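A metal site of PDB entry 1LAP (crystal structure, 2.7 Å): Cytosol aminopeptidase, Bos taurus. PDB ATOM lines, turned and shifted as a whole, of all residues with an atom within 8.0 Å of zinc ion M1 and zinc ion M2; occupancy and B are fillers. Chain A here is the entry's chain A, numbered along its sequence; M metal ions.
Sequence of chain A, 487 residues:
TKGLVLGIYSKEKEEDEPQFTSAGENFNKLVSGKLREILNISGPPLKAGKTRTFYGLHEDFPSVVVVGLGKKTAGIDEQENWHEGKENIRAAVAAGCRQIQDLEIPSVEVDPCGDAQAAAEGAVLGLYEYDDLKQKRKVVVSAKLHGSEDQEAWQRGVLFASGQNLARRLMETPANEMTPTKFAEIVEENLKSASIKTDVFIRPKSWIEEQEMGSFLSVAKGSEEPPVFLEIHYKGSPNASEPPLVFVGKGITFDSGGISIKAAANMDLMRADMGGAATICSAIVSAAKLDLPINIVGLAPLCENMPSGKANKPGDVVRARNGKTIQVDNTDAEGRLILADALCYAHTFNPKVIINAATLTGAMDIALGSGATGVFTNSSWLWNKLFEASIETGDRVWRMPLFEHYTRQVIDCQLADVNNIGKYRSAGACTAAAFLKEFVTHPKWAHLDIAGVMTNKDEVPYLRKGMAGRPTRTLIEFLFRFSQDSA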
ATOM      1  N   VAL A 219     -11.005 -21.727  -6.996  1.00  0.00           N
ATOM      2  CA  VAL A 219     -12.075 -20.767  -6.818  1.00  0.00           C
ATOM      3  C   VAL A 219     -13.359 -21.544  -6.676  1.00  0.00           C
ATOM      4  O   VAL A 219     -14.073 -21.368  -5.682  1.00  0.00           O
ATOM      5  CB  VAL A 219     -12.196 -19.826  -8.019  1.00  0.00           C
ATOM      6  CG1 VAL A 219     -13.395 -18.897  -7.871  1.00  0.00           C
ATOM      7  CG2 VAL A 219     -10.975 -18.926  -8.040  1.00  0.00           C
ATOM      8  N   LYS A 250     -14.021 -14.043 -18.304  1.00  0.00           N
ATOM      9  CA  LYS A 250     -14.198 -14.425 -16.915  1.00  0.00           C
ATOM     10  C   LYS A 250     -15.694 -14.730 -16.747  1.00  0.00           C
ATOM     11  O   LYS A 250     -16.518 -13.860 -17.079  1.00  0.00           O
ATOM     12  CB  LYS A 250     -13.755 -13.232 -16.047  1.00  0.00           C
ATOM     13  CG  LYS A 250     -14.019 -13.312 -14.522  1.00  0.00           C
ATOM     14  CD  LYS A 250     -13.629 -12.029 -13.845  1.00  0.00           C
ATOM     15  CE  LYS A 250     -14.076 -12.275 -12.453  1.00  0.00           C
ATOM     16  NZ  LYS A 250     -14.108 -11.056 -11.672  1.00  0.00           N
ATOM     17  N   GLY A 251     -16.086 -15.925 -16.317  1.00  0.00           N
ATOM     18  CA  GLY A 251     -17.464 -16.209 -16.060  1.00  0.00           C
ATOM     19  C   GLY A 251     -17.686 -16.502 -14.601  1.00  0.00           C
ATOM     20  O   GLY A 251     -17.933 -17.663 -14.220  1.00  0.00           O
ATOM     21  N   ILE A 252     -17.591 -15.495 -13.714  1.00  0.00           N
ATOM     22  CA  ILE A 252     -17.919 -15.794 -12.328  1.00  0.00           C
ATOM     23  C   ILE A 252     -19.404 -15.510 -12.316  1.00  0.00           C
ATOM     24  O   ILE A 252     -19.801 -14.449 -12.766  1.00  0.00           O
ATOM     25  CB  ILE A 252     -17.107 -14.905 -11.341  1.00  0.00           C
ATOM     26  CG1 ILE A 252     -15.655 -15.325 -11.523  1.00  0.00           C
ATOM     27  CG2 ILE A 252     -17.453 -15.129  -9.844  1.00  0.00           C
ATOM     28  CD1 ILE A 252     -15.300 -16.724 -10.950  1.00  0.00           C
ATOM     29  N   THR A 253     -20.284 -16.430 -11.902  1.00  0.00           N
ATOM     30  CA  THR A 253     -21.692 -16.199 -12.062  1.00  0.00           C
ATOM     31  C   THR A 253     -22.316 -15.480 -10.911  1.00  0.00           C
ATOM     32  O   THR A 253     -23.401 -14.911 -10.992  1.00  0.00           O
ATOM     33  CB  THR A 253     -22.349 -17.568 -12.366  1.00  0.00           C
ATOM     34  OG1 THR A 253     -21.918 -18.554 -11.442  1.00  0.00           O
ATOM     35  CG2 THR A 253     -21.980 -17.975 -13.840  1.00  0.00           C
ATOM     36  N   PHE A 254     -21.586 -15.519  -9.817  1.00  0.00           N
ATOM     37  CA  PHE A 254     -21.867 -14.652  -8.702  1.00  0.00           C
ATOM     38  C   PHE A 254     -20.574 -14.580  -7.933  1.00  0.00           C
ATOM     39  O   PHE A 254     -19.937 -15.616  -7.627  1.00  0.00           O
ATOM     40  CB  PHE A 254     -22.941 -15.195  -7.710  1.00  0.00           C
ATOM     41  CG  PHE A 254     -23.211 -14.125  -6.629  1.00  0.00           C
ATOM     42  CD1 PHE A 254     -23.780 -12.922  -7.006  1.00  0.00           C
ATOM     43  CD2 PHE A 254     -22.791 -14.334  -5.328  1.00  0.00           C
ATOM     44  CE1 PHE A 254     -23.855 -11.893  -6.115  1.00  0.00           C
ATOM     45  CE2 PHE A 254     -22.902 -13.325  -4.411  1.00  0.00           C
ATOM     46  CZ  PHE A 254     -23.413 -12.105  -4.818  1.00  0.00           C
ATOM     47  N   ASP A 255     -20.229 -13.347  -7.580  1.00  0.00           N
ATOM     48  CA  ASP A 255     -19.065 -13.185  -6.718  1.00  0.00           C
ATOM     49  C   ASP A 255     -19.411 -12.593  -5.362  1.00  0.00           C
ATOM     50  O   ASP A 255     -19.787 -11.405  -5.229  1.00  0.00           O
ATOM     51  CB  ASP A 255     -18.062 -12.316  -7.404  1.00  0.00           C
ATOM     52  CG  ASP A 255     -16.717 -12.171  -6.736  1.00  0.00           C
ATOM     53  OD1 ASP A 255     -16.093 -11.227  -7.176  1.00  0.00           O
ATOM     54  OD2 ASP A 255     -16.311 -12.936  -5.857  1.00  0.00           O
ATOM     55  N   SER A 256     -19.267 -13.447  -4.356  1.00  0.00           N
ATOM     56  CA  SER A 256     -19.527 -12.961  -3.014  1.00  0.00           C
ATOM     57  C   SER A 256     -18.268 -12.378  -2.427  1.00  0.00           C
ATOM     58  O   SER A 256     -18.344 -11.672  -1.429  1.00  0.00           O
ATOM     59  CB  SER A 256     -20.008 -14.080  -2.102  1.00  0.00           C
ATOM     60  OG  SER A 256     -18.981 -15.065  -2.010  1.00  0.00           O
ATOM     61  N   GLY A 257     -17.104 -12.737  -2.998  1.00  0.00           N
ATOM     62  CA  GLY A 257     -15.791 -12.413  -2.415  1.00  0.00           C
ATOM     63  C   GLY A 257     -15.069 -13.642  -1.801  1.00  0.00           C
ATOM     64  O   GLY A 257     -13.822 -13.772  -1.731  1.00  0.00           O
ATOM     65  N   GLY A 258     -15.877 -14.639  -1.436  1.00  0.00           N
ATOM     66  CA  GLY A 258     -15.370 -15.795  -0.775  1.00  0.00           C
ATOM     67  C   GLY A 258     -15.220 -15.390   0.677  1.00  0.00           C
ATOM     68  O   GLY A 258     -16.108 -14.715   1.219  1.00  0.00           O
ATOM     69  N   SER A 260     -12.629 -13.597   1.765  1.00  0.00           N
ATOM     70  CA  SER A 260     -12.454 -12.139   1.729  1.00  0.00           C
ATOM     71  C   SER A 260     -13.815 -11.534   1.270  1.00  0.00           C
ATOM     72  O   SER A 260     -13.927 -10.847   0.233  1.00  0.00           O
ATOM     73  CB  SER A 260     -11.373 -11.831   0.763  1.00  0.00           C
ATOM     74  OG  SER A 260     -10.233 -12.696   0.870  1.00  0.00           O
ATOM     75  N   LYS A 262     -17.243  -9.708   0.342  1.00  0.00           N
ATOM     76  CA  LYS A 262     -17.649  -8.423  -0.135  1.00  0.00           C
ATOM     77  C   LYS A 262     -18.500  -7.679   0.903  1.00  0.00           C
ATOM     78  O   LYS A 262     -19.101  -8.274   1.805  1.00  0.00           O
ATOM     79  CB  LYS A 262     -18.442  -8.628  -1.392  1.00  0.00           C
ATOM     80  CG  LYS A 262     -17.854  -8.087  -2.683  1.00  0.00           C
ATOM     81  CD  LYS A 262     -17.573  -9.234  -3.598  1.00  0.00           C
ATOM     82  CE  LYS A 262     -17.247  -8.814  -5.013  1.00  0.00           C
ATOM     83  NZ  LYS A 262     -16.096  -7.926  -5.061  1.00  0.00           N
ATOM     84  N   MET A 270     -22.951  -8.347  -8.499  1.00  0.00           N
ATOM     85  CA  MET A 270     -21.932  -9.308  -8.880  1.00  0.00           C
ATOM     86  C   MET A 270     -22.573 -10.492  -9.605  1.00  0.00           C
ATOM     87  O   MET A 270     -21.903 -11.443 -10.007  1.00  0.00           O
ATOM     88  CB  MET A 270     -21.164  -9.768  -7.645  1.00  0.00           C
ATOM     89  CG  MET A 270     -20.287  -8.712  -6.977  1.00  0.00           C
ATOM     90  SD  MET A 270     -19.354  -7.619  -8.090  1.00  0.00           S
ATOM     91  CE  MET A 270     -17.862  -8.500  -8.295  1.00  0.00           C
ATOM     92  N   ALA A 272     -23.390  -9.889 -12.323  1.00  0.00           N
ATOM     93  CA  ALA A 272     -22.773  -9.531 -13.552  1.00  0.00           C
ATOM     94  C   ALA A 272     -21.292  -9.750 -13.632  1.00  0.00           C
ATOM     95  O   ALA A 272     -20.698  -9.273 -14.607  1.00  0.00           O
ATOM     96  CB  ALA A 272     -23.045  -8.104 -13.833  1.00  0.00           C
ATOM     97  N   ASP A 273     -20.683 -10.565 -12.749  1.00  0.00           N
ATOM     98  CA  ASP A 273     -19.260 -10.831 -12.793  1.00  0.00           C
ATOM     99  C   ASP A 273     -18.955 -11.873 -13.890  1.00  0.00           C
ATOM    100  O   ASP A 273     -17.884 -12.461 -14.009  1.00  0.00           O
ATOM    101  CB  ASP A 273     -18.815 -11.314 -11.390  1.00  0.00           C
ATOM    102  CG  ASP A 273     -17.391 -10.879 -11.052  1.00  0.00           C
ATOM    103  OD1 ASP A 273     -16.657 -11.613 -10.380  1.00  0.00           O
ATOM    104  OD2 ASP A 273     -17.006  -9.788 -11.476  1.00  0.00           O
ATOM    105  N   MET A 274     -19.936 -12.263 -14.670  1.00  0.00           N
ATOM    106  CA  MET A 274     -19.672 -13.149 -15.783  1.00  0.00           C
ATOM    107  C   MET A 274     -19.821 -12.323 -17.053  1.00  0.00           C
ATOM    108  O   MET A 274     -19.804 -12.884 -18.151  1.00  0.00           O
ATOM    109  CB  MET A 274     -20.641 -14.381 -15.798  1.00  0.00           C
ATOM    110  CG  MET A 274     -22.069 -14.105 -15.283  1.00  0.00           C
ATOM    111  SD  MET A 274     -22.970 -12.765 -16.120  1.00  0.00           S
ATOM    112  CE  MET A 274     -23.175 -13.729 -17.579  1.00  0.00           C
ATOM    113  N   ASN A 305     -18.173 -17.702  -6.803  1.00  0.00           N
ATOM    114  CA  ASN A 305     -17.172 -17.588  -5.750  1.00  0.00           C
ATOM    115  C   ASN A 305     -17.861 -17.373  -4.409  1.00  0.00           C
ATOM    116  O   ASN A 305     -18.320 -16.280  -4.136  1.00  0.00           O
ATOM    117  CB  ASN A 305     -16.226 -16.446  -6.088  1.00  0.00           C
ATOM    118  CG  ASN A 305     -15.154 -16.181  -5.033  1.00  0.00           C
ATOM    119  OD1 ASN A 305     -14.771 -15.051  -4.776  1.00  0.00           O
ATOM    120  ND2 ASN A 305     -14.606 -17.179  -4.368  1.00  0.00           N
ATOM    121  N   ASN A 330      -5.927 -12.734  -1.319  1.00  0.00           N
ATOM    122  CA  ASN A 330      -7.261 -12.218  -1.156  1.00  0.00           C
ATOM    123  C   ASN A 330      -8.113 -13.078  -2.100  1.00  0.00           C
ATOM    124  O   ASN A 330      -7.844 -13.206  -3.317  1.00  0.00           O
ATOM    125  CB  ASN A 330      -7.246 -10.742  -1.539  1.00  0.00           C
ATOM    126  CG  ASN A 330      -8.605 -10.177  -1.906  1.00  0.00           C
ATOM    127  OD1 ASN A 330      -9.609 -10.489  -1.298  1.00  0.00           O
ATOM    128  ND2 ASN A 330      -8.750  -9.377  -2.951  1.00  0.00           N
ATOM    129  N   THR A 331      -9.169 -13.660  -1.547  1.00  0.00           N
ATOM    130  CA  THR A 331     -10.019 -14.576  -2.315  1.00  0.00           C
ATOM    131  C   THR A 331     -10.959 -13.855  -3.290  1.00  0.00           C
ATOM    132  O   THR A 331     -11.505 -14.468  -4.207  1.00  0.00           O
ATOM    133  CB  THR A 331     -10.816 -15.515  -1.325  1.00  0.00           C
ATOM    134  OG1 THR A 331     -11.665 -14.739  -0.497  1.00  0.00           O
ATOM    135  CG2 THR A 331      -9.907 -16.194  -0.324  1.00  0.00           C
ATOM    136  N   ASP A 332     -11.112 -12.517  -3.087  1.00  0.00           N
ATOM    137  CA  ASP A 332     -11.935 -11.709  -3.986  1.00  0.00           C
ATOM    138  C   ASP A 332     -11.139 -11.388  -5.261  1.00  0.00           C
ATOM    139  O   ASP A 332     -11.657 -10.857  -6.212  1.00  0.00           O
ATOM    140  CB  ASP A 332     -12.393 -10.430  -3.249  1.00  0.00           C
ATOM    141  CG  ASP A 332     -13.583  -9.684  -3.851  1.00  0.00           C
ATOM    142  OD1 ASP A 332     -13.774  -8.527  -3.482  1.00  0.00           O
ATOM    143  OD2 ASP A 332     -14.315 -10.241  -4.658  1.00  0.00           O
ATOM    144  N   ALA A 333      -9.846 -11.731  -5.363  1.00  0.00           N
ATOM    145  CA  ALA A 333      -9.111 -11.528  -6.611  1.00  0.00           C
ATOM    146  C   ALA A 333      -9.121 -12.899  -7.319  1.00  0.00           C
ATOM    147  O   ALA A 333      -8.131 -13.477  -7.768  1.00  0.00           O
ATOM    148  CB  ALA A 333      -7.693 -11.057  -6.291  1.00  0.00           C
ATOM    149  N   GLU A 334     -10.364 -13.411  -7.450  1.00  0.00           N
ATOM    150  CA  GLU A 334     -10.564 -14.713  -8.059  1.00  0.00           C
ATOM    151  C   GLU A 334     -10.547 -14.792  -9.589  1.00  0.00           C
ATOM    152  O   GLU A 334     -10.043 -15.738 -10.170  1.00  0.00           O
ATOM    153  CB  GLU A 334     -11.883 -15.339  -7.502  1.00  0.00           C
ATOM    154  CG  GLU A 334     -13.251 -15.101  -8.194  1.00  0.00           C
ATOM    155  CD  GLU A 334     -13.665 -13.647  -8.159  1.00  0.00           C
ATOM    156  OE1 GLU A 334     -14.181 -13.151  -9.145  1.00  0.00           O
ATOM    157  OE2 GLU A 334     -13.425 -13.052  -7.121  1.00  0.00           O
ATOM    158  N   GLY A 335     -11.144 -13.882 -10.337  1.00  0.00           N
ATOM    159  CA  GLY A 335     -11.079 -13.882 -11.785  1.00  0.00           C
ATOM    160  C   GLY A 335      -9.723 -14.029 -12.407  1.00  0.00           C
ATOM    161  O   GLY A 335      -9.621 -14.705 -13.425  1.00  0.00           O
ATOM    162  N   ARG A 336      -8.747 -13.381 -11.767  1.00  0.00           N
ATOM    163  CA  ARG A 336      -7.304 -13.447 -12.003  1.00  0.00           C
ATOM    164  C   ARG A 336      -6.963 -14.950 -12.083  1.00  0.00           C
ATOM    165  O   ARG A 336      -6.445 -15.518 -13.060  1.00  0.00           O
ATOM    166  CB  ARG A 336      -6.541 -12.781 -10.784  1.00  0.00           C
ATOM    167  CG  ARG A 336      -6.072 -11.306 -10.773  1.00  0.00           C
ATOM    168  CD  ARG A 336      -6.296 -10.345  -9.559  1.00  0.00           C
ATOM    169  NE  ARG A 336      -7.462  -9.433  -9.616  1.00  0.00           N
ATOM    170  CZ  ARG A 336      -8.774  -9.836  -9.812  1.00  0.00           C
ATOM    171  NH1 ARG A 336      -9.778  -8.982  -9.944  1.00  0.00           N
ATOM    172  NH2 ARG A 336      -9.196 -11.104  -9.865  1.00  0.00           N
ATOM    173  N   ILE A 338      -8.848 -17.571 -12.264  1.00  0.00           N
ATOM    174  CA  ILE A 338      -9.612 -18.356 -13.251  1.00  0.00           C
ATOM    175  C   ILE A 338      -9.069 -18.245 -14.679  1.00  0.00           C
ATOM    176  O   ILE A 338      -8.817 -19.226 -15.412  1.00  0.00           O
ATOM    177  CB  ILE A 338     -11.055 -17.871 -12.983  1.00  0.00           C
ATOM    178  CG1 ILE A 338     -11.535 -19.106 -12.322  1.00  0.00           C
ATOM    179  CG2 ILE A 338     -11.991 -17.403 -14.097  1.00  0.00           C
ATOM    180  CD1 ILE A 338     -12.587 -18.750 -11.280  1.00  0.00           C
ATOM    181  N   ALA A 358     -12.971  -9.262 -18.872  1.00  0.00           N
ATOM    182  CA  ALA A 358     -13.276  -9.505 -17.480  1.00  0.00           C
ATOM    183  C   ALA A 358     -13.701  -8.255 -16.734  1.00  0.00           C
ATOM    184  O   ALA A 358     -13.171  -7.177 -16.923  1.00  0.00           O
ATOM    185  CB  ALA A 358     -12.067 -10.046 -16.779  1.00  0.00           C
ATOM    186  N   THR A 359     -14.661  -8.387 -15.828  1.00  0.00           N
ATOM    187  CA  THR A 359     -15.145  -7.359 -14.950  1.00  0.00           C
ATOM    188  C   THR A 359     -14.125  -7.594 -13.839  1.00  0.00           C
ATOM    189  O   THR A 359     -14.420  -8.173 -12.799  1.00  0.00           O
ATOM    190  CB  THR A 359     -16.606  -7.702 -14.527  1.00  0.00           C
ATOM    191  OG1 THR A 359     -16.638  -9.115 -14.497  1.00  0.00           O
ATOM    192  CG2 THR A 359     -17.701  -7.170 -15.445  1.00  0.00           C
ATOM    193  N   LEU A 360     -12.880  -7.189 -14.055  1.00  0.00           N
ATOM    194  CA  LEU A 360     -11.863  -7.575 -13.115  1.00  0.00           C
ATOM    195  C   LEU A 360     -11.757  -6.744 -11.882  1.00  0.00           C
ATOM    196  O   LEU A 360     -11.708  -7.256 -10.781  1.00  0.00           O
ATOM    197  CB  LEU A 360     -10.483  -7.550 -13.738  1.00  0.00           C
ATOM    198  CG  LEU A 360      -9.701  -8.822 -13.947  1.00  0.00           C
ATOM    199  CD1 LEU A 360      -8.265  -8.457 -13.634  1.00  0.00           C
ATOM    200  CD2 LEU A 360     -10.222  -9.999 -13.122  1.00  0.00           C
ATOM    201  N   THR A 361     -11.847  -5.427 -12.045  1.00  0.00           N
ATOM    202  CA  THR A 361     -11.324  -4.602 -11.024  1.00  0.00           C
ATOM    203  C   THR A 361     -12.159  -3.389 -10.832  1.00  0.00           C
ATOM    204  O   THR A 361     -12.395  -2.713 -11.799  1.00  0.00           O
ATOM    205  CB  THR A 361      -9.877  -4.447 -11.584  1.00  0.00           C
ATOM    206  OG1 THR A 361      -9.090  -4.923 -10.547  1.00  0.00           O
ATOM    207  CG2 THR A 361      -9.425  -3.090 -12.002  1.00  0.00           C
HETATM  208 ZN    ZN M   1     -14.810 -11.320  -9.538  1.00  0.00          ZN
HETATM  209 ZN    ZN M   2     -13.999 -11.174  -6.768  1.00  0.00          ZN
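Within 4 Å of zinc ion M2: Asp 255, Asp 332 and Glu 334.
Zinc ion M2 is bound by OE2 of Glu 334 (2.0 Å), OD1 of Asp 255 (2.1 Å), OD2 of Asp 332 (2.3 Å) and O of Asp 332 (2.4 Å).
Zinc ion M2 has four donor atoms within binding distance.
OD1 of Asp 255 sits close to NZ of Lys 262.
The side-chain carboxylate of Asp 273 is in hydrogen-bond range of the side-chain hydroxyl of Thr 359 (3.1 Å).
OD1 of Asp 332 is in salt-bridge range of NZ of Lys 262, at 2.9 Å.
O of Gly 257 lies within hydrogen-bond range of N of Asp 332 (3.3 Å).
OD1 of Asn 305 lies close to OD2 of Asp 255 (2.8 Å).
The side-chain carboxylate (OD2) of Asp 255 is in hydrogen-bond range of the backbone NH (N) of Gly 257, 3.0 Å away.
The side-chain carboxylate of Glu 334 lies close to the side-chain amide oxygen of Asn 305 (3.4 Å).
O of Asp 273 lies within hydrogen-bond range of N of Ile 252, 3.1 Å away.
Zinc ion M1 is bound by the side-chain carboxylate of Glu 334 (2.0 Å), the side-chain carboxylate of Asp 273 (2.1 Å) and the side-chain amino group of Lys 250 (2.3 Å).
Slightly farther from zinc ion M1 lies OD1 of Asp 255 (2.7 Å).
Of the 29 residues printed, 4 come within 4 Å of zinc ion M1.
The nearest printed residue that does not touch zinc ion M1 is Met 270 (4.3 Å).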
